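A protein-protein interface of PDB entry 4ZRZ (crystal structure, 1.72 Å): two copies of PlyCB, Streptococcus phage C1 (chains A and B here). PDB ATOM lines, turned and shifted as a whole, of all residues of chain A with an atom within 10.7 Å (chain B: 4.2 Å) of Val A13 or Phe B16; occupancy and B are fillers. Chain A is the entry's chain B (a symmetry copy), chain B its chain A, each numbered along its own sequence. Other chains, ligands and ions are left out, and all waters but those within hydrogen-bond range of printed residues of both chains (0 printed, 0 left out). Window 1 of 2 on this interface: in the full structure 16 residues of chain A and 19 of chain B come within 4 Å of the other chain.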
ATOM      1  N   ASN A   9      23.106  23.922  -2.637  1.00  0.00           N
ATOM      2  CA  ASN A   9      21.991  24.633  -1.924  1.00  0.00           C
ATOM      3  C   ASN A   9      20.696  23.815  -1.955  1.00  0.00           C
ATOM      4  O   ASN A   9      20.299  23.227  -0.931  1.00  0.00           O
ATOM      5  CB  ASN A   9      21.790  26.038  -2.526  1.00  0.00           C
ATOM      6  CG  ASN A   9      20.652  26.806  -1.879  1.00  0.00           C
ATOM      7  OD1 ASN A   9      19.784  27.341  -2.568  1.00  0.00           O
ATOM      8  ND2 ASN A   9      20.658  26.874  -0.552  1.00  0.00           N
ATOM      9  N   VAL A  10      20.096  23.745  -3.152  1.00  0.00           N
ATOM     10  CA  VAL A  10      18.806  23.070  -3.407  1.00  0.00           C
ATOM     11  C   VAL A  10      18.759  21.568  -3.064  1.00  0.00           C
ATOM     12  O   VAL A  10      17.681  21.031  -2.797  1.00  0.00           O
ATOM     13  CB  VAL A  10      18.374  23.268  -4.888  1.00  0.00           C
ATOM     14  CG1 VAL A  10      19.293  22.534  -5.866  1.00  0.00           C
ATOM     15  CG2 VAL A  10      16.948  22.827  -5.094  1.00  0.00           C
ATOM     16  N   SER A  11      19.909  20.900  -3.072  1.00  0.00           N
ATOM     17  CA  SER A  11      19.965  19.444  -2.797  1.00  0.00           C
ATOM     18  C   SER A  11      19.779  19.062  -1.346  1.00  0.00           C
ATOM     19  O   SER A  11      19.534  17.900  -1.041  1.00  0.00           O
ATOM     20  CB  SER A  11      21.304  18.901  -3.242  1.00  0.00           C
ATOM     21  OG  SER A  11      22.300  19.466  -2.393  1.00  0.00           O
ATOM     22  N   GLY A  12      19.960  20.014  -0.429  1.00  0.00           N
ATOM     23  CA  GLY A  12      19.959  19.714   0.961  1.00  0.00           C
ATOM     24  C   GLY A  12      21.178  18.926   1.394  1.00  0.00           C
ATOM     25  O   GLY A  12      21.158  18.329   2.445  1.00  0.00           O
ATOM     26  N   VAL A  13      22.241  18.949   0.601  1.00  0.00           N
ATOM     27  CA  VAL A  13      23.467  18.179   0.904  1.00  0.00           C
ATOM     28  C   VAL A  13      24.661  19.118   0.778  1.00  0.00           C
ATOM     29  O   VAL A  13      24.863  19.718  -0.283  1.00  0.00           O
ATOM     30  CB  VAL A  13      23.666  17.014  -0.081  1.00  0.00           C
ATOM     31  CG1 VAL A  13      24.963  16.249   0.237  1.00  0.00           C
ATOM     32  CG2 VAL A  13      22.468  16.070  -0.076  1.00  0.00           C
ATOM     33  N   GLN A  14      25.423  19.240   1.863  1.00  0.00           N
ATOM     34  CA  GLN A  14      26.745  19.846   1.832  1.00  0.00           C
ATOM     35  C   GLN A  14      27.750  18.744   2.157  1.00  0.00           C
ATOM     36  O   GLN A  14      27.584  18.029   3.148  1.00  0.00           O
ATOM     37  CB  GLN A  14      26.890  20.938   2.879  1.00  0.00           C
ATOM     38  CG  GLN A  14      26.251  22.266   2.514  1.00  0.00           C
ATOM     39  CD  GLN A  14      26.660  23.346   3.502  1.00  0.00           C
ATOM     40  OE1 GLN A  14      26.832  23.077   4.693  1.00  0.00           O
ATOM     41  NE2 GLN A  14      26.856  24.554   3.010  1.00  0.00           N
ATOM     42  N   GLY A  15      28.812  18.678   1.384  1.00  0.00           N
ATOM     43  CA  GLY A  15      29.873  17.693   1.652  1.00  0.00           C
ATOM     44  C   GLY A  15      30.695  17.335   0.456  1.00  0.00           C
ATOM     45  O   GLY A  15      30.690  18.029  -0.555  1.00  0.00           O
ATOM     46  N   PHE A  16      31.386  16.199   0.553  1.00  0.00           N
ATOM     47  CA  PHE A  16      32.216  15.760  -0.536  1.00  0.00           C
ATOM     48  C   PHE A  16      32.494  14.254  -0.439  1.00  0.00           C
ATOM     49  O   PHE A  16      32.443  13.688   0.639  1.00  0.00           O
ATOM     50  CB  PHE A  16      33.533  16.561  -0.582  1.00  0.00           C
ATOM     51  CG  PHE A  16      34.378  16.413   0.654  1.00  0.00           C
ATOM     52  CD1 PHE A  16      35.383  15.440   0.716  1.00  0.00           C
ATOM     53  CD2 PHE A  16      34.182  17.235   1.749  1.00  0.00           C
ATOM     54  CE1 PHE A  16      36.160  15.292   1.852  1.00  0.00           C
ATOM     55  CE2 PHE A  16      34.960  17.102   2.888  1.00  0.00           C
ATOM     56  CZ  PHE A  16      35.956  16.113   2.935  1.00  0.00           C
ATOM     57  N   LEU A  17      32.761  13.671  -1.598  1.00  0.00           N
ATOM     58  CA  LEU A  17      33.267  12.314  -1.728  1.00  0.00           C
ATOM     59  C   LEU A  17      34.790  12.362  -1.631  1.00  0.00           C
ATOM     60  O   LEU A  17      35.438  13.282  -2.155  1.00  0.00           O
ATOM     61  CB  LEU A  17      32.885  11.746  -3.078  1.00  0.00           C
ATOM     62  CG  LEU A  17      31.385  11.512  -3.318  1.00  0.00           C
ATOM     63  CD1 LEU A  17      30.997  11.621  -4.764  1.00  0.00           C
ATOM     64  CD2 LEU A  17      31.054  10.121  -2.816  1.00  0.00           C
ATOM     65  N   ALA A  30      32.340   9.522   2.050  1.00  0.00           N
ATOM     66  CA  ALA A  30      31.747  10.871   1.900  1.00  0.00           C
ATOM     67  C   ALA A  30      31.493  11.466   3.256  1.00  0.00           C
ATOM     68  O   ALA A  30      31.201  10.731   4.193  1.00  0.00           O
ATOM     69  CB  ALA A  30      30.430  10.808   1.146  1.00  0.00           C
ATOM     70  N   PHE A  31      31.571  12.794   3.331  1.00  0.00           N
ATOM     71  CA  PHE A  31      30.987  13.555   4.405  1.00  0.00           C
ATOM     72  C   PHE A  31      29.726  14.146   3.815  1.00  0.00           C
ATOM     73  O   PHE A  31      29.797  14.776   2.792  1.00  0.00           O
ATOM     74  CB  PHE A  31      31.905  14.681   4.872  1.00  0.00           C
ATOM     75  CG  PHE A  31      32.965  14.201   5.784  1.00  0.00           C
ATOM     76  CD1 PHE A  31      32.695  14.020   7.128  1.00  0.00           C
ATOM     77  CD2 PHE A  31      34.215  13.866   5.284  1.00  0.00           C
ATOM     78  CE1 PHE A  31      33.678  13.538   7.977  1.00  0.00           C
ATOM     79  CE2 PHE A  31      35.200  13.386   6.123  1.00  0.00           C
ATOM     80  CZ  PHE A  31      34.933  13.221   7.461  1.00  0.00           C
ATOM     81  N   ILE A  32      28.592  13.845   4.441  1.00  0.00           N
ATOM     82  CA  ILE A  32      27.263  14.331   4.022  1.00  0.00           C
ATOM     83  C   ILE A  32      26.658  15.022   5.236  1.00  0.00           C
ATOM     84  O   ILE A  32      26.355  14.352   6.241  1.00  0.00           O
ATOM     85  CB  ILE A  32      26.330  13.156   3.633  1.00  0.00           C
ATOM     86  CG1 ILE A  32      26.936  12.276   2.538  1.00  0.00           C
ATOM     87  CG2 ILE A  32      24.933  13.658   3.238  1.00  0.00           C
ATOM     88  CD1 ILE A  32      27.016  12.895   1.174  1.00  0.00           C
ATOM     89  N   ASN A  33      26.480  16.340   5.139  1.00  0.00           N
ATOM     90  CA  ASN A  33      25.968  17.152   6.255  1.00  0.00           C
ATOM     91  C   ASN A  33      26.646  16.808   7.586  1.00  0.00           C
ATOM     92  O   ASN A  33      25.992  16.559   8.602  1.00  0.00           O
ATOM     93  CB  ASN A  33      24.429  17.041   6.328  1.00  0.00           C
ATOM     94  CG  ASN A  33      23.742  17.489   5.041  1.00  0.00           C
ATOM     95  OD1 ASN A  33      24.274  18.304   4.290  1.00  0.00           O
ATOM     96  ND2 ASN A  33      22.557  16.926   4.763  1.00  0.00           N
ATOM     97  N   GLY A  34      27.977  16.753   7.536  1.00  0.00           N
ATOM     98  CA  GLY A  34      28.808  16.522   8.701  1.00  0.00           C
ATOM     99  C   GLY A  34      28.889  15.092   9.184  1.00  0.00           C
ATOM    100  O   GLY A  34      29.470  14.853  10.234  1.00  0.00           O
ATOM    101  N   VAL A  35      28.303  14.143   8.452  1.00  0.00           N
ATOM    102  CA  VAL A  35      28.300  12.734   8.864  1.00  0.00           C
ATOM    103  C   VAL A  35      29.150  11.969   7.871  1.00  0.00           C
ATOM    104  O   VAL A  35      28.930  12.071   6.673  1.00  0.00           O
ATOM    105  CB  VAL A  35      26.874  12.144   8.879  1.00  0.00           C
ATOM    106  CG1 VAL A  35      26.884  10.673   9.291  1.00  0.00           C
ATOM    107  CG2 VAL A  35      25.975  12.949   9.810  1.00  0.00           C
ATOM    108  N   ILE A  37      30.281   8.658   5.930  1.00  0.00           N
ATOM    109  CA  ILE A  37      29.754   7.359   5.497  1.00  0.00           C
ATOM    110  C   ILE A  37      30.669   6.698   4.485  1.00  0.00           C
ATOM    111  O   ILE A  37      31.475   7.355   3.806  1.00  0.00           O
ATOM    112  CB  ILE A  37      28.339   7.442   4.854  1.00  0.00           C
ATOM    113  CG1 ILE A  37      28.322   8.360   3.637  1.00  0.00           C
ATOM    114  CG2 ILE A  37      27.310   7.880   5.884  1.00  0.00           C
ATOM    115  CD1 ILE A  37      27.002   8.323   2.889  1.00  0.00           C
ATOM    116  N   ILE A  39      30.642   4.531   0.964  1.00  0.00           N
ATOM    117  CA  ILE A  39      29.814   4.294  -0.224  1.00  0.00           C
ATOM    118  C   ILE A  39      30.248   2.956  -0.812  1.00  0.00           C
ATOM    119  O   ILE A  39      31.434   2.766  -1.112  1.00  0.00           O
ATOM    120  CB  ILE A  39      30.034   5.370  -1.311  1.00  0.00           C
ATOM    121  CG1 ILE A  39      29.866   6.780  -0.765  1.00  0.00           C
ATOM    122  CG2 ILE A  39      29.125   5.126  -2.506  1.00  0.00           C
ATOM    123  CD1 ILE A  39      28.506   7.106  -0.221  1.00  0.00           C
ATOM    124  N   THR A  44      26.262   4.911  -6.881  1.00  0.00           N
ATOM    125  CA  THR A  44      26.008   5.905  -5.852  1.00  0.00           C
ATOM    126  C   THR A  44      27.082   7.013  -5.896  1.00  0.00           C
ATOM    127  O   THR A  44      26.788   8.192  -5.762  1.00  0.00           O
ATOM    128  CB  THR A  44      26.016   5.241  -4.478  1.00  0.00           C
ATOM    129  OG1 THR A  44      25.097   4.146  -4.489  1.00  0.00           O
ATOM    130  CG2 THR A  44      25.637   6.230  -3.371  1.00  0.00           C
ATOM    131  N   GLY A  47      26.097   9.156  -8.859  1.00  0.00           N
ATOM    132  CA  GLY A  47      24.904   9.941  -8.393  1.00  0.00           C
ATOM    133  C   GLY A  47      25.316  11.162  -7.577  1.00  0.00           C
ATOM    134  O   GLY A  47      24.918  12.295  -7.888  1.00  0.00           O
ATOM    135  N   PHE A  48      26.116  10.944  -6.540  1.00  0.00           N
ATOM    136  CA  PHE A  48      26.545  12.055  -5.681  1.00  0.00           C
ATOM    137  C   PHE A  48      27.482  13.039  -6.336  1.00  0.00           C
ATOM    138  O   PHE A  48      27.427  14.240  -6.021  1.00  0.00           O
ATOM    139  CB  PHE A  48      27.071  11.588  -4.339  1.00  0.00           C
ATOM    140  CG  PHE A  48      25.969  11.302  -3.357  1.00  0.00           C
ATOM    141  CD1 PHE A  48      25.410  12.337  -2.612  1.00  0.00           C
ATOM    142  CD2 PHE A  48      25.407  10.040  -3.260  1.00  0.00           C
ATOM    143  CE1 PHE A  48      24.365  12.098  -1.737  1.00  0.00           C
ATOM    144  CE2 PHE A  48      24.360   9.791  -2.386  1.00  0.00           C
ATOM    145  CZ  PHE A  48      23.828  10.827  -1.629  1.00  0.00           C
ATOM    146  N   GLN A  49      28.257  12.568  -7.301  1.00  0.00           N
ATOM    147  CA  GLN A  49      29.090  13.452  -8.123  1.00  0.00           C
ATOM    148  C   GLN A  49      28.288  14.480  -8.948  1.00  0.00           C
ATOM    149  O   GLN A  49      28.848  15.477  -9.388  1.00  0.00           O
ATOM    150  CB  GLN A  49      30.005  12.637  -9.011  1.00  0.00           C
ATOM    151  CG  GLN A  49      31.183  12.043  -8.248  1.00  0.00           C
ATOM    152  CD  GLN A  49      32.046  11.109  -9.089  1.00  0.00           C
ATOM    153  OE1 GLN A  49      31.624  10.598 -10.139  1.00  0.00           O
ATOM    154  NE2 GLN A  49      33.273  10.865  -8.617  1.00  0.00           N
ATOM    155  N   GLN A  50      26.989  14.239  -9.149  1.00  0.00           N
ATOM    156  CA  GLN A  50      26.120  15.257  -9.772  1.00  0.00           C
ATOM    157  C   GLN A  50      25.859  16.431  -8.831  1.00  0.00           C
ATOM    158  O   GLN A  50      25.481  17.530  -9.307  1.00  0.00           O
ATOM    159  CB  GLN A  50      24.770  14.653 -10.198  1.00  0.00           C
ATOM    160  CG  GLN A  50      24.872  13.446 -11.113  1.00  0.00           C
ATOM    161  CD  GLN A  50      25.206  13.791 -12.551  1.00  0.00           C
ATOM    162  OE1 GLN A  50      26.289  14.301 -12.870  1.00  0.00           O
ATOM    163  N   ILE A  51      25.958  16.251  -7.516  1.00  0.00           N
ATOM    164  CA  ILE A  51      25.568  17.316  -6.563  1.00  0.00           C
ATOM    165  C   ILE A  51      26.658  17.784  -5.575  1.00  0.00           C
ATOM    166  O   ILE A  51      26.535  18.849  -4.972  1.00  0.00           O
ATOM    167  CB  ILE A  51      24.310  16.946  -5.750  1.00  0.00           C
ATOM    168  CG1 ILE A  51      24.503  15.641  -4.971  1.00  0.00           C
ATOM    169  CG2 ILE A  51      23.108  16.839  -6.669  1.00  0.00           C
ATOM    170  CD1 ILE A  51      23.490  15.433  -3.863  1.00  0.00           C
ATOM    171  N   ILE A  52      27.704  16.983  -5.364  1.00  0.00           N
ATOM    172  CA  ILE A  52      28.780  17.380  -4.454  1.00  0.00           C
ATOM    173  C   ILE A  52      30.130  17.053  -5.081  1.00  0.00           C
ATOM    174  O   ILE A  52      30.216  16.167  -5.934  1.00  0.00           O
ATOM    175  CB  ILE A  52      28.698  16.743  -3.059  1.00  0.00           C
ATOM    176  CG1 ILE A  52      28.645  15.209  -3.130  1.00  0.00           C
ATOM    177  CG2 ILE A  52      27.536  17.323  -2.245  1.00  0.00           C
ATOM    178  CD1 ILE A  52      28.624  14.551  -1.778  1.00  0.00           C
ATOM    179  N   PRO A  53      31.172  17.779  -4.660  1.00  0.00           N
ATOM    180  CA  PRO A  53      32.467  17.527  -5.260  1.00  0.00           C
ATOM    181  C   PRO A  53      33.025  16.176  -4.841  1.00  0.00           C
ATOM    182  O   PRO A  53      32.640  15.602  -3.807  1.00  0.00           O
ATOM    183  CB  PRO A  53      33.365  18.651  -4.692  1.00  0.00           C
ATOM    184  CG  PRO A  53      32.626  19.249  -3.576  1.00  0.00           C
ATOM    185  CD  PRO A  53      31.177  18.972  -3.785  1.00  0.00           C
ATOM    186  N   MET A  69      36.863  17.561  10.395  1.00  0.00           N
ATOM    187  CA  MET A  69      35.445  17.578  10.067  1.00  0.00           C
ATOM    188  C   MET A  69      34.531  17.233  11.277  1.00  0.00           C
ATOM    189  O   MET A  69      33.314  17.141  11.110  1.00  0.00           O
ATOM    190  CB  MET A  69      35.168  16.647   8.870  1.00  0.00           C
ATOM    191  CG  MET A  69      35.855  17.044   7.560  1.00  0.00           C
ATOM    192  SD  MET A  69      35.283  18.565   6.758  1.00  0.00           S
ATOM    193  CE  MET A  69      33.509  18.311   6.626  1.00  0.00           C
ATOM    194  N   GLY B  15      16.387  18.992  -1.238  1.00  0.00           N
ATOM    195  CA  GLY B  15      16.520  17.531  -1.238  1.00  0.00           C
ATOM    196  C   GLY B  15      16.787  17.009  -2.628  1.00  0.00           C
ATOM    197  O   GLY B  15      17.255  17.719  -3.488  1.00  0.00           O
ATOM    198  N   PHE B  16      16.493  15.731  -2.846  1.00  0.00           N
ATOM    199  CA  PHE B  16      16.718  15.113  -4.130  1.00  0.00           C
ATOM    200  C   PHE B  16      15.828  13.863  -4.275  1.00  0.00           C
ATOM    201  O   PHE B  16      15.420  13.283  -3.279  1.00  0.00           O
ATOM    202  CB  PHE B  16      18.203  14.737  -4.303  1.00  0.00           C
ATOM    203  CG  PHE B  16      18.761  13.894  -3.182  1.00  0.00           C
ATOM    204  CD1 PHE B  16      18.669  12.503  -3.200  1.00  0.00           C
ATOM    205  CD2 PHE B  16      19.408  14.491  -2.101  1.00  0.00           C
ATOM    206  CE1 PHE B  16      19.176  11.734  -2.166  1.00  0.00           C
ATOM    207  CE2 PHE B  16      19.932  13.717  -1.059  1.00  0.00           C
ATOM    208  CZ  PHE B  16      19.817  12.331  -1.094  1.00  0.00           C
ATOM    209  N   LEU B  17      15.535  13.525  -5.514  1.00  0.00           N
ATOM    210  CA  LEU B  17      14.980  12.218  -5.889  1.00  0.00           C
ATOM    211  C   LEU B  17      16.129  11.228  -5.988  1.00  0.00           C
ATOM    212  O   LEU B  17      17.261  11.596  -6.401  1.00  0.00           O
ATOM    213  CB  LEU B  17      14.305  12.315  -7.241  1.00  0.00           C
ATOM    214  CG  LEU B  17      13.016  13.152  -7.254  1.00  0.00           C
ATOM    215  CD1 LEU B  17      12.849  13.855  -8.572  1.00  0.00           C
ATOM    216  CD2 LEU B  17      11.803  12.262  -6.988  1.00  0.00           C
ATOM    217  N   PHE B  18      15.833   9.965  -5.669  1.00  0.00           N
ATOM    218  CA  PHE B  18      16.798   8.900  -5.866  1.00  0.00           C
ATOM    219  C   PHE B  18      16.131   7.608  -6.340  1.00  0.00           C
ATOM    220  O   PHE B  18      14.983   7.340  -6.002  1.00  0.00           O
ATOM    221  CB  PHE B  18      17.708   8.698  -4.636  1.00  0.00           C
ATOM    222  CG  PHE B  18      17.006   8.382  -3.330  1.00  0.00           C
ATOM    223  CD1 PHE B  18      17.092   7.103  -2.757  1.00  0.00           C
ATOM    224  CD2 PHE B  18      16.348   9.373  -2.605  1.00  0.00           C
ATOM    225  CE1 PHE B  18      16.526   6.825  -1.514  1.00  0.00           C
ATOM    226  CE2 PHE B  18      15.765   9.090  -1.370  1.00  0.00           C
ATOM    227  CZ  PHE B  18      15.869   7.838  -0.812  1.00  0.00           C
ATOM    228  N   ALA B  30      12.477  10.069  -2.464  1.00  0.00           N
ATOM    229  CA  ALA B  30      13.018  11.426  -2.295  1.00  0.00           C
ATOM    230  C   ALA B  30      13.253  11.758  -0.851  1.00  0.00           C
ATOM    231  O   ALA B  30      12.575  11.240   0.023  1.00  0.00           O
ATOM    232  CB  ALA B  30      12.080  12.426  -2.913  1.00  0.00           C
ATOM    233  N   PHE B  31      14.241  12.627  -0.607  1.00  0.00           N
ATOM    234  CA  PHE B  31      14.338  13.404   0.627  1.00  0.00           C
ATOM    235  C   PHE B  31      13.787  14.799   0.342  1.00  0.00           C
ATOM    236  O   PHE B  31      14.215  15.451  -0.602  1.00  0.00           O
ATOM    237  CB  PHE B  31      15.789  13.485   1.151  1.00  0.00           C
ATOM    238  CG  PHE B  31      16.275  12.190   1.736  1.00  0.00           C
ATOM    239  CD1 PHE B  31      15.904  11.820   3.016  1.00  0.00           C
ATOM    240  CD2 PHE B  31      17.046  11.328   0.993  1.00  0.00           C
ATOM    241  CE1 PHE B  31      16.317  10.603   3.546  1.00  0.00           C
ATOM    242  CE2 PHE B  31      17.462  10.118   1.506  1.00  0.00           C
ATOM    243  CZ  PHE B  31      17.095   9.758   2.788  1.00  0.00           C
ATOM    244  N   ILE B  52      14.117  19.991  -7.826  1.00  0.00           N
ATOM    245  CA  ILE B  52      15.222  19.348  -7.066  1.00  0.00           C
ATOM    246  C   ILE B  52      15.997  18.366  -7.941  1.00  0.00           C
ATOM    247  O   ILE B  52      15.439  17.825  -8.916  1.00  0.00           O
ATOM    248  CB  ILE B  52      14.756  18.684  -5.749  1.00  0.00           C
ATOM    249  CG1 ILE B  52      13.732  17.540  -5.996  1.00  0.00           C
ATOM    250  CG2 ILE B  52      14.216  19.734  -4.785  1.00  0.00           C
ATOM    251  CD1 ILE B  52      13.329  16.744  -4.768  1.00  0.00           C
ATOM    252  N   PRO B  53      17.280  18.120  -7.597  1.00  0.00           N
ATOM    253  CA  PRO B  53      18.065  17.192  -8.390  1.00  0.00           C
ATOM    254  C   PRO B  53      17.520  15.764  -8.317  1.00  0.00           C
ATOM    255  O   PRO B  53      16.869  15.387  -7.323  1.00  0.00           O
ATOM    256  CB  PRO B  53      19.484  17.269  -7.771  1.00  0.00           C
ATOM    257  CG  PRO B  53      19.384  18.114  -6.547  1.00  0.00           C
ATOM    258  CD  PRO B  53      18.093  18.863  -6.605  1.00  0.00           C
ATOM    259  N   ILE B  55      19.107  11.964  -8.644  1.00  0.00           N
ATOM    260  CA  ILE B  55      20.366  11.206  -8.670  1.00  0.00           C
ATOM    261  C   ILE B  55      20.151   9.706  -8.511  1.00  0.00           C
ATOM    262  O   ILE B  55      19.068   9.265  -8.162  1.00  0.00           O
ATOM    263  CB  ILE B  55      21.364  11.749  -7.624  1.00  0.00           C
ATOM    264  CG1 ILE B  55      20.926  11.442  -6.184  1.00  0.00           C
ATOM    265  CG2 ILE B  55      21.592  13.231  -7.891  1.00  0.00           C
ATOM    266  CD1 ILE B  55      21.995  11.723  -5.145  1.00  0.00           C
ATOM    267  N   ILE B  57      21.219   6.183  -6.597  1.00  0.00           N
ATOM    268  CA  ILE B  57      21.750   5.617  -5.368  1.00  0.00           C
ATOM    269  C   ILE B  57      21.449   4.134  -5.420  1.00  0.00           C
ATOM    270  O   ILE B  57      20.297   3.760  -5.588  1.00  0.00           O
ATOM    271  CB  ILE B  57      21.122   6.219  -4.101  1.00  0.00           C
ATOM    272  CG1 ILE B  57      21.320   7.748  -4.059  1.00  0.00           C
ATOM    273  CG2 ILE B  57      21.679   5.575  -2.850  1.00  0.00           C
ATOM    274  CD1 ILE B  57      20.770   8.398  -2.791  1.00  0.00           C
ATOM    275  N   ILE B  65      22.853   6.583   3.373  1.00  0.00           N
ATOM    276  CA  ILE B  65      22.360   7.909   3.002  1.00  0.00           C
ATOM    277  C   ILE B  65      21.283   8.410   3.987  1.00  0.00           C
ATOM    278  O   ILE B  65      21.340   9.558   4.444  1.00  0.00           O
ATOM    279  CB  ILE B  65      21.862   7.957   1.541  1.00  0.00           C
ATOM    280  CG1 ILE B  65      23.015   7.620   0.578  1.00  0.00           C
ATOM    281  CG2 ILE B  65      21.296   9.340   1.211  1.00  0.00           C
ATOM    282  CD1 ILE B  65      24.251   8.491   0.733  1.00  0.00           C
ATOM    283  N   MET B  69      21.050  11.813   6.031  1.00  0.00           N
ATOM    284  CA  MET B  69      19.927  12.704   5.735  1.00  0.00           C
ATOM    285  C   MET B  69      18.863  12.624   6.858  1.00  0.00           C
ATOM    286  O   MET B  69      17.677  12.869   6.608  1.00  0.00           O
ATOM    287  CB  MET B  69      19.329  12.359   4.359  1.00  0.00           C
ATOM    288  CG  MET B  69      20.294  12.475   3.188  1.00  0.00           C
ATOM    289  SD  MET B  69      20.872  14.146   2.778  1.00  0.00           S
ATOM    290  CE  MET B  69      19.339  14.914   2.242  1.00  0.00           C
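The backbone NH of Gly B15 sits at hydrogen-bond distance from the backbone carbonyl oxygen of Val A10, 2.9 Å away. N of Gly B15 lies close to O of Ser A11 (3.3 Å).
O of Ala A30 sits at hydrogen-bond distance from N of Ile A37. The side-chain hydroxyl (OG) of Ser A11 lies within hydrogen-bond range of the backbone NH (N) of Val A13 (3.0 Å). The backbone NH of Phe B31 is in hydrogen-bond range of the backbone carbonyl oxygen of Phe B16, at 3.0 Å. O of Gln A14 is in hydrogen-bond range of N of Asn A33. The backbone carbonyl oxygen of Leu B17 lies within hydrogen-bond range of the backbone NH of Ile B55, 2.9 Å away. O of Pro B53 lies within hydrogen-bond range of N of Leu B17, at 2.9 Å.
Phe B16 touches Ser A11. Ser A11 touches Pro B53 (CB to CG, 3.9 Å). N of Gly A12 touches N of Gly B15, 3.8 Å away. Gly A12 touches Met B69. Met B69 touches Val A13. Ile B65 touches Ile A37. Thr A44 touches Ile B57. Gly A47 touches Ile B55. CZ of Phe A48 touches CD1 of Ile B65, 3.3 Å away. Pro B53 touches Ile A51.
Phe B16 touches just these residues of chain A: Ser A11 and Val A13. Of the printed residues of chain A, Gly B15 touches Val A10, Ser A11 and Gly A12. No residue of chain A comes within 4 Å of Leu B17. No residue of chain A comes within 4 Å of Ala B30. No residue of chain A comes within 4 Å of Phe B31. No residue of chain A comes within 4 Å of Ile B52. Of chain A, only Gly A47 (3.5 Å) comes within 4 Å of Ile B55. Of the printed residues of chain B, Thr A44 touches Ile B57. Printed residues of chain B within 4 Å of Ile A51: Pro B53. The nearest printed residue of chain B that does not touch Val A13 is Gly B15 (6.1 Å).
Of the 12 printed residues of chain B, 7 touch a printed residue of chain A. Printed residues of chain B that touch a printed residue of chain A: Gly B15, Phe B16, Pro B53, Ile B55, Ile B57, Ile B65 and Met B69. Hydrophobic or aromatic side chains of chain B within 4 Å of the printed part of chain A: Phe B16, Pro B53, Ile B55, Ile B57, Ile B65 and Met B69. Printed residues of chain A that touch a printed residue of chain B: Val A10, Ser A11, Gly A12, Val A13, Asn A33, Ile A37, Thr A44, Gly A47, Phe A48 and Ile A51. Hydrophobic or aromatic side chains of chain A that line the printed part of chain B: Val A10, Val A13, Ile A37, Phe A48 and Ile A51. Among the printed residues, no Asp or Glu carboxylate lies within 4 Å of a Lys or Arg side-chain nitrogen of the other chain.
Positions printed for both chains: 15, 16, 17, 30, 31, 52, 53 and 69. Of the 16 pairs that touch across the chains among the printed residues, none has its exchanged pair printed and touching as well.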
